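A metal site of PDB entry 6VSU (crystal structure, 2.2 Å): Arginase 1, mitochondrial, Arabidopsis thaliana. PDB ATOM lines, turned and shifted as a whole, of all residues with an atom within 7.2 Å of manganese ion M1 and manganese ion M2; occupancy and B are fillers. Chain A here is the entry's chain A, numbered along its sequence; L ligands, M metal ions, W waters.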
ATOM      1  N   ASP A 139      17.872   6.993 -16.541  1.00  0.00           N
ATOM      2  CA  ASP A 139      18.297   8.115 -17.405  1.00  0.00           C
ATOM      3  C   ASP A 139      19.179   7.573 -18.534  1.00  0.00           C
ATOM      4  O   ASP A 139      19.563   6.410 -18.494  1.00  0.00           O
ATOM      5  CB  ASP A 139      18.958   9.224 -16.595  1.00  0.00           C
ATOM      6  CG  ASP A 139      20.320   8.921 -16.000  1.00  0.00           C
ATOM      7  OD1 ASP A 139      21.183   8.391 -16.729  1.00  0.00           O
ATOM      8  OD2 ASP A 139      20.509   9.283 -14.820  1.00  0.00           O
ATOM      9  N   HIS A 140      19.566   8.432 -19.458  1.00  0.00           N
ATOM     10  CA  HIS A 140      20.196   8.009 -20.720  1.00  0.00           C
ATOM     11  C   HIS A 140      21.646   7.584 -20.475  1.00  0.00           C
ATOM     12  O   HIS A 140      22.208   6.944 -21.375  1.00  0.00           O
ATOM     13  CB  HIS A 140      20.050   9.100 -21.789  1.00  0.00           C
ATOM     14  CG  HIS A 140      19.827   8.521 -23.142  1.00  0.00           C
ATOM     15  ND1 HIS A 140      19.055   9.148 -24.074  1.00  0.00           N
ATOM     16  CD2 HIS A 140      20.216   7.333 -23.663  1.00  0.00           C
ATOM     17  CE1 HIS A 140      18.988   8.406 -25.152  1.00  0.00           C
ATOM     18  NE2 HIS A 140      19.694   7.255 -24.926  1.00  0.00           N
ATOM     19  N   SER A 141      22.249   7.875 -19.306  1.00  0.00           N
ATOM     20  CA  SER A 141      23.640   7.426 -19.029  1.00  0.00           C
ATOM     21  C   SER A 141      23.702   5.905 -19.178  1.00  0.00           C
ATOM     22  O   SER A 141      24.769   5.403 -19.549  1.00  0.00           O
ATOM     23  CB  SER A 141      24.139   7.903 -17.699  1.00  0.00           C
ATOM     24  OG  SER A 141      23.335   7.414 -16.624  1.00  0.00           O
ATOM     25  N   HIS A 162      19.195   5.944 -32.688  1.00  0.00           N
ATOM     26  CA  HIS A 162      19.118   6.697 -31.419  1.00  0.00           C
ATOM     27  C   HIS A 162      17.984   7.681 -31.567  1.00  0.00           C
ATOM     28  O   HIS A 162      18.206   8.680 -32.262  1.00  0.00           O
ATOM     29  CB  HIS A 162      20.494   7.333 -31.126  1.00  0.00           C
ATOM     30  CG  HIS A 162      20.461   8.306 -29.998  1.00  0.00           C
ATOM     31  ND1 HIS A 162      21.366   9.357 -29.923  1.00  0.00           N
ATOM     32  CD2 HIS A 162      19.646   8.403 -28.938  1.00  0.00           C
ATOM     33  CE1 HIS A 162      21.073  10.066 -28.837  1.00  0.00           C
ATOM     34  NE2 HIS A 162      20.026   9.505 -28.225  1.00  0.00           N
ATOM     35  N   LEU A 163      16.823   7.412 -30.969  1.00  0.00           N
ATOM     36  CA  LEU A 163      15.664   8.343 -31.002  1.00  0.00           C
ATOM     37  C   LEU A 163      15.673   9.260 -29.766  1.00  0.00           C
ATOM     38  O   LEU A 163      15.547   8.782 -28.618  1.00  0.00           O
ATOM     39  CB  LEU A 163      14.396   7.488 -31.068  1.00  0.00           C
ATOM     40  CG  LEU A 163      14.178   6.717 -32.383  1.00  0.00           C
ATOM     41  CD1 LEU A 163      13.212   5.563 -32.200  1.00  0.00           C
ATOM     42  CD2 LEU A 163      13.641   7.644 -33.420  1.00  0.00           C
ATOM     43  N   ASP A 164      15.786  10.582 -29.977  1.00  0.00           N
ATOM     44  CA  ASP A 164      15.963  11.538 -28.865  1.00  0.00           C
ATOM     45  C   ASP A 164      15.789  12.966 -29.378  1.00  0.00           C
ATOM     46  O   ASP A 164      16.170  13.237 -30.525  1.00  0.00           O
ATOM     47  CB  ASP A 164      17.344  11.304 -28.276  1.00  0.00           C
ATOM     48  CG  ASP A 164      17.536  11.780 -26.848  1.00  0.00           C
ATOM     49  OD1 ASP A 164      16.917  12.793 -26.460  1.00  0.00           O
ATOM     50  OD2 ASP A 164      18.286  11.106 -26.123  1.00  0.00           O
ATOM     51  N   ALA A 165      15.188  13.850 -28.577  1.00  0.00           N
ATOM     52  CA  ALA A 165      15.243  15.307 -28.798  1.00  0.00           C
ATOM     53  C   ALA A 165      16.691  15.801 -28.791  1.00  0.00           C
ATOM     54  O   ALA A 165      16.975  16.836 -29.459  1.00  0.00           O
ATOM     55  CB  ALA A 165      14.453  16.051 -27.778  1.00  0.00           C
ATOM     56  N   HIS A 166      17.554  15.115 -28.035  1.00  0.00           N
ATOM     57  CA  HIS A 166      18.934  15.582 -27.722  1.00  0.00           C
ATOM     58  C   HIS A 166      19.962  14.586 -28.267  1.00  0.00           C
ATOM     59  O   HIS A 166      19.736  13.380 -28.274  1.00  0.00           O
ATOM     60  CB  HIS A 166      19.084  15.723 -26.181  1.00  0.00           C
ATOM     61  CG  HIS A 166      17.949  16.454 -25.509  1.00  0.00           C
ATOM     62  ND1 HIS A 166      16.856  15.785 -25.035  1.00  0.00           N
ATOM     63  CD2 HIS A 166      17.768  17.783 -25.239  1.00  0.00           C
ATOM     64  CE1 HIS A 166      16.024  16.687 -24.522  1.00  0.00           C
ATOM     65  NE2 HIS A 166      16.578  17.917 -24.622  1.00  0.00           N
ATOM     66  N   PRO A 167      21.169  15.045 -28.683  1.00  0.00           N
ATOM     67  CA  PRO A 167      22.161  14.107 -29.201  1.00  0.00           C
ATOM     68  C   PRO A 167      22.986  13.367 -28.120  1.00  0.00           C
ATOM     69  O   PRO A 167      23.561  12.338 -28.445  1.00  0.00           O
ATOM     70  CB  PRO A 167      23.006  14.977 -30.133  1.00  0.00           C
ATOM     71  CG  PRO A 167      22.875  16.387 -29.599  1.00  0.00           C
ATOM     72  CD  PRO A 167      21.588  16.447 -28.808  1.00  0.00           C
ATOM     73  N   ASP A 168      23.014  13.877 -26.881  1.00  0.00           N
ATOM     74  CA  ASP A 168      23.670  13.228 -25.711  1.00  0.00           C
ATOM     75  C   ASP A 168      25.131  12.911 -26.066  1.00  0.00           C
ATOM     76  O   ASP A 168      25.628  11.807 -25.815  1.00  0.00           O
ATOM     77  CB  ASP A 168      22.871  12.005 -25.243  1.00  0.00           C
ATOM     78  CG  ASP A 168      21.499  12.374 -24.698  1.00  0.00           C
ATOM     79  OD1 ASP A 168      21.263  13.573 -24.438  1.00  0.00           O
ATOM     80  OD2 ASP A 168      20.689  11.433 -24.497  1.00  0.00           O
ATOM     81  N   HIS A 180      24.019  11.829 -18.419  1.00  0.00           N
ATOM     82  CA  HIS A 180      23.029  11.330 -19.407  1.00  0.00           C
ATOM     83  C   HIS A 180      23.167  12.096 -20.741  1.00  0.00           C
ATOM     84  O   HIS A 180      22.551  11.670 -21.736  1.00  0.00           O
ATOM     85  CB  HIS A 180      21.610  11.437 -18.829  1.00  0.00           C
ATOM     86  CG  HIS A 180      21.039  12.800 -18.653  1.00  0.00           C
ATOM     87  ND1 HIS A 180      19.666  12.983 -18.511  1.00  0.00           N
ATOM     88  CD2 HIS A 180      21.575  14.025 -18.557  1.00  0.00           C
ATOM     89  CE1 HIS A 180      19.395  14.273 -18.354  1.00  0.00           C
ATOM     90  NE2 HIS A 180      20.533  14.929 -18.398  1.00  0.00           N
ATOM     91  N   ALA A 181      23.882  13.226 -20.744  1.00  0.00           N
ATOM     92  CA  ALA A 181      24.066  14.076 -21.920  1.00  0.00           C
ATOM     93  C   ALA A 181      25.404  13.752 -22.574  1.00  0.00           C
ATOM     94  O   ALA A 181      25.749  14.513 -23.454  1.00  0.00           O
ATOM     95  CB  ALA A 181      23.988  15.530 -21.531  1.00  0.00           C
ATOM     96  N   SER A 183      26.328  10.068 -22.977  1.00  0.00           N
ATOM     97  CA  SER A 183      26.304   8.594 -23.184  1.00  0.00           C
ATOM     98  C   SER A 183      26.861   8.255 -24.573  1.00  0.00           C
ATOM     99  O   SER A 183      27.555   7.275 -24.709  1.00  0.00           O
ATOM    100  CB  SER A 183      24.921   7.973 -23.015  1.00  0.00           C
ATOM    101  OG  SER A 183      24.178   8.664 -22.043  1.00  0.00           O
ATOM    102  N   PHE A 184      26.512   9.065 -25.573  1.00  0.00           N
ATOM    103  CA  PHE A 184      26.810   8.784 -26.999  1.00  0.00           C
ATOM    104  C   PHE A 184      28.249   9.208 -27.331  1.00  0.00           C
ATOM    105  O   PHE A 184      28.839   8.548 -28.167  1.00  0.00           O
ATOM    106  CB  PHE A 184      25.675   9.311 -27.873  1.00  0.00           C
ATOM    107  CG  PHE A 184      24.473   8.419 -27.732  1.00  0.00           C
ATOM    108  CD1 PHE A 184      24.385   7.224 -28.437  1.00  0.00           C
ATOM    109  CD2 PHE A 184      23.502   8.690 -26.788  1.00  0.00           C
ATOM    110  CE1 PHE A 184      23.316   6.364 -28.250  1.00  0.00           C
ATOM    111  CE2 PHE A 184      22.425   7.849 -26.615  1.00  0.00           C
ATOM    112  CZ  PHE A 184      22.329   6.680 -27.346  1.00  0.00           C
ATOM    113  N   SER A 247      18.252   2.710 -29.204  1.00  0.00           N
ATOM    114  CA  SER A 247      18.058   3.484 -27.945  1.00  0.00           C
ATOM    115  C   SER A 247      16.880   4.447 -28.118  1.00  0.00           C
ATOM    116  O   SER A 247      16.903   5.239 -29.057  1.00  0.00           O
ATOM    117  CB  SER A 247      19.296   4.221 -27.546  1.00  0.00           C
ATOM    118  OG  SER A 247      19.031   4.986 -26.380  1.00  0.00           O
ATOM    119  N   ILE A 248      15.892   4.416 -27.241  1.00  0.00           N
ATOM    120  CA  ILE A 248      14.743   5.353 -27.378  1.00  0.00           C
ATOM    121  C   ILE A 248      14.614   6.209 -26.122  1.00  0.00           C
ATOM    122  O   ILE A 248      14.305   5.649 -25.062  1.00  0.00           O
ATOM    123  CB  ILE A 248      13.435   4.609 -27.661  1.00  0.00           C
ATOM    124  CG1 ILE A 248      13.612   3.674 -28.864  1.00  0.00           C
ATOM    125  CG2 ILE A 248      12.303   5.624 -27.857  1.00  0.00           C
ATOM    126  CD1 ILE A 248      12.356   2.950 -29.214  1.00  0.00           C
ATOM    127  N   ASP A 249      14.904   7.485 -26.259  1.00  0.00           N
ATOM    128  CA  ASP A 249      14.588   8.537 -25.250  1.00  0.00           C
ATOM    129  C   ASP A 249      13.125   8.922 -25.514  1.00  0.00           C
ATOM    130  O   ASP A 249      12.797   9.433 -26.626  1.00  0.00           O
ATOM    131  CB  ASP A 249      15.529   9.729 -25.368  1.00  0.00           C
ATOM    132  CG  ASP A 249      15.350  10.804 -24.295  1.00  0.00           C
ATOM    133  OD1 ASP A 249      14.185  10.962 -23.804  1.00  0.00           O
ATOM    134  OD2 ASP A 249      16.363  11.500 -24.027  1.00  0.00           O
ATOM    135  N   VAL A 250      12.286   8.630 -24.559  1.00  0.00           N
ATOM    136  CA  VAL A 250      10.849   9.000 -24.612  1.00  0.00           C
ATOM    137  C   VAL A 250      10.678  10.479 -25.068  1.00  0.00           C
ATOM    138  O   VAL A 250       9.685  10.745 -25.789  1.00  0.00           O
ATOM    139  CB  VAL A 250      10.256   8.675 -23.236  1.00  0.00           C
ATOM    140  CG1 VAL A 250       8.911   9.328 -23.003  1.00  0.00           C
ATOM    141  CG2 VAL A 250      10.123   7.166 -23.102  1.00  0.00           C
ATOM    142  N   ASP A 251      11.625  11.380 -24.791  1.00  0.00           N
ATOM    143  CA  ASP A 251      11.483  12.795 -25.269  1.00  0.00           C
ATOM    144  C   ASP A 251      11.722  12.909 -26.792  1.00  0.00           C
ATOM    145  O   ASP A 251      11.698  14.077 -27.326  1.00  0.00           O
ATOM    146  CB  ASP A 251      12.339  13.770 -24.448  1.00  0.00           C
ATOM    147  CG  ASP A 251      13.830  13.688 -24.661  1.00  0.00           C
ATOM    148  OD1 ASP A 251      14.265  13.273 -25.770  1.00  0.00           O
ATOM    149  OD2 ASP A 251      14.571  13.977 -23.662  1.00  0.00           O
ATOM    150  N   CYS A 252      11.894  11.790 -27.524  1.00  0.00           N
ATOM    151  CA  CYS A 252      11.875  11.841 -29.003  1.00  0.00           C
ATOM    152  C   CYS A 252      10.481  12.264 -29.455  1.00  0.00           C
ATOM    153  O   CYS A 252      10.382  12.916 -30.515  1.00  0.00           O
ATOM    154  CB  CYS A 252      12.316  10.553 -29.692  1.00  0.00           C
ATOM    155  SG  CYS A 252      11.161   9.168 -29.534  1.00  0.00           S
ATOM    156  N   HIS A 263      12.930  16.720 -19.749  1.00  0.00           N
ATOM    157  CA  HIS A 263      13.195  17.800 -20.733  1.00  0.00           C
ATOM    158  C   HIS A 263      12.036  17.975 -21.714  1.00  0.00           C
ATOM    159  O   HIS A 263      12.048  17.332 -22.759  1.00  0.00           O
ATOM    160  CB  HIS A 263      14.502  17.473 -21.415  1.00  0.00           C
ATOM    161  CG  HIS A 263      15.592  17.367 -20.402  1.00  0.00           C
ATOM    162  ND1 HIS A 263      16.365  18.437 -20.046  1.00  0.00           N
ATOM    163  CD2 HIS A 263      15.998  16.308 -19.658  1.00  0.00           C
ATOM    164  CE1 HIS A 263      17.201  18.058 -19.095  1.00  0.00           C
ATOM    165  NE2 HIS A 263      16.989  16.742 -18.820  1.00  0.00           N
ATOM    166  N   VAL A 291      14.325   4.790 -22.294  1.00  0.00           N
ATOM    167  CA  VAL A 291      14.960   5.523 -21.162  1.00  0.00           C
ATOM    168  C   VAL A 291      14.261   6.867 -21.031  1.00  0.00           C
ATOM    169  O   VAL A 291      13.520   7.240 -21.929  1.00  0.00           O
ATOM    170  CB  VAL A 291      16.466   5.714 -21.361  1.00  0.00           C
ATOM    171  CG1 VAL A 291      17.194   4.408 -21.617  1.00  0.00           C
ATOM    172  CG2 VAL A 291      16.750   6.692 -22.484  1.00  0.00           C
ATOM    173  N   GLU A 292      14.494   7.530 -19.908  1.00  0.00           N
ATOM    174  CA  GLU A 292      14.109   8.943 -19.631  1.00  0.00           C
ATOM    175  C   GLU A 292      12.602   9.130 -19.477  1.00  0.00           C
ATOM    176  O   GLU A 292      12.156  10.270 -19.510  1.00  0.00           O
ATOM    177  CB  GLU A 292      14.651   9.884 -20.695  1.00  0.00           C
ATOM    178  CG  GLU A 292      16.133  10.032 -20.621  1.00  0.00           C
ATOM    179  CD  GLU A 292      16.729  10.778 -19.449  1.00  0.00           C
ATOM    180  OE1 GLU A 292      15.956  11.380 -18.678  1.00  0.00           O
ATOM    181  OE2 GLU A 292      17.995  10.734 -19.317  1.00  0.00           O
HETATM  182  N1  LIG L   1      20.148  20.795 -21.282  1.00  0.00           N
HETATM  183  C1  LIG L   1      20.779  19.530 -21.786  1.00  0.00           C
HETATM  184  C2  LIG L   1      19.750  18.381 -21.797  1.00  0.00           C
HETATM  185  C3  LIG L   1      20.336  16.989 -21.899  1.00  0.00           C
HETATM  186  C4  LIG L   1      19.277  15.903 -21.888  1.00  0.00           C
HETATM  187  N2  LIG L   1      19.758  14.516 -21.851  1.00  0.00           N
HETATM  188  C5  LIG L   1      21.325  19.784 -23.202  1.00  0.00           C
HETATM  189  O1  LIG L   1      21.268  18.897 -24.061  1.00  0.00           O
HETATM  190  O2  LIG L   1      21.832  20.870 -23.522  1.00  0.00           O
HETATM  191 MN    MN M   1      16.430  13.557 -24.630  1.00  0.00          MN
HETATM  192 MN    MN M   2      18.798  11.421 -24.232  1.00  0.00          MN
HETATM  193  O   HOH W   1      17.007  13.551 -21.681  1.00  0.00           O
HETATM  194  O   HOH W   2      18.240  13.708 -23.788  1.00  0.00           O
HETATM  195  O   HOH W   3      19.749  12.097 -22.162  1.00  0.00           O
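The side-chain carboxylate of Asp 168 lies within salt-bridge range of a nitrogen (N2) of the ligand (3.1 Å).
The backbone carbonyl oxygen (O) of Asp 168 is in hydrogen-bond range of the backbone NH (N) of Phe 184. The backbone NH of Ser 183 is in hydrogen-bond range of the backbone carbonyl oxygen of Asp 168, 3.4 Å away. A ring nitrogen (NE2) of His 162 lies close to the side-chain carboxylate (OD2) of Asp 164 (3.2 Å). The side-chain carboxylate (OD1) of Asp 251 lies close to the backbone NH (N) of Ala 165, 3.0 Å away. The side-chain sulfur (SG) of Cys 252 lies close to the backbone carbonyl oxygen (O) of Asp 249 (3.3 Å). OE2 of Glu 292 sits at hydrogen-bond distance from N of His 140 (2.8 Å). The side-chain hydroxyl (OG) of Ser 183 lies within hydrogen-bond range of the backbone carbonyl oxygen (O) of His 140 (2.7 Å). OG of Ser 247 lies within hydrogen-bond range of NE2 of His 140 (2.8 Å).
The nearest printed residue that does not touch manganese ion M1 is Ala 165 (4.1 Å).
Four residues have an atom within 4 Å of manganese ion M2: His 140, Asp 164, Asp 168 and Asp 249. The nearest printed residue that does not touch manganese ion M2 is His 180 (4.5 Å).
Manganese ion M1 is bound by water W2, OD1 of Asp 164, OD2 of Asp 251, OD2 of Asp 249, ND1 of His 166 and OD1 of Asp 251.
Manganese ion M2 is bound by OD2 of Asp 168 (1.9 Å), OD2 of Asp 164 (2.0 Å), ND1 of His 140 (2.3 Å), water W3 (2.4 Å), water W2 (2.4 Å) and OD2 of Asp 249 (2.4 Å). Manganese ion M2 has six donor atoms within binding distance.
Water W2 bridges a nitrogen (N2) of the ligand (2.6 Å) and the side-chain carboxylate of Asp 168 (3.1 Å). Water W3 lies within hydrogen-bond range of a nitrogen (N2) of the ligand, the backbone carbonyl oxygen (O) of His 180 and the side-chain carboxylate (OD1) of Asp 168.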
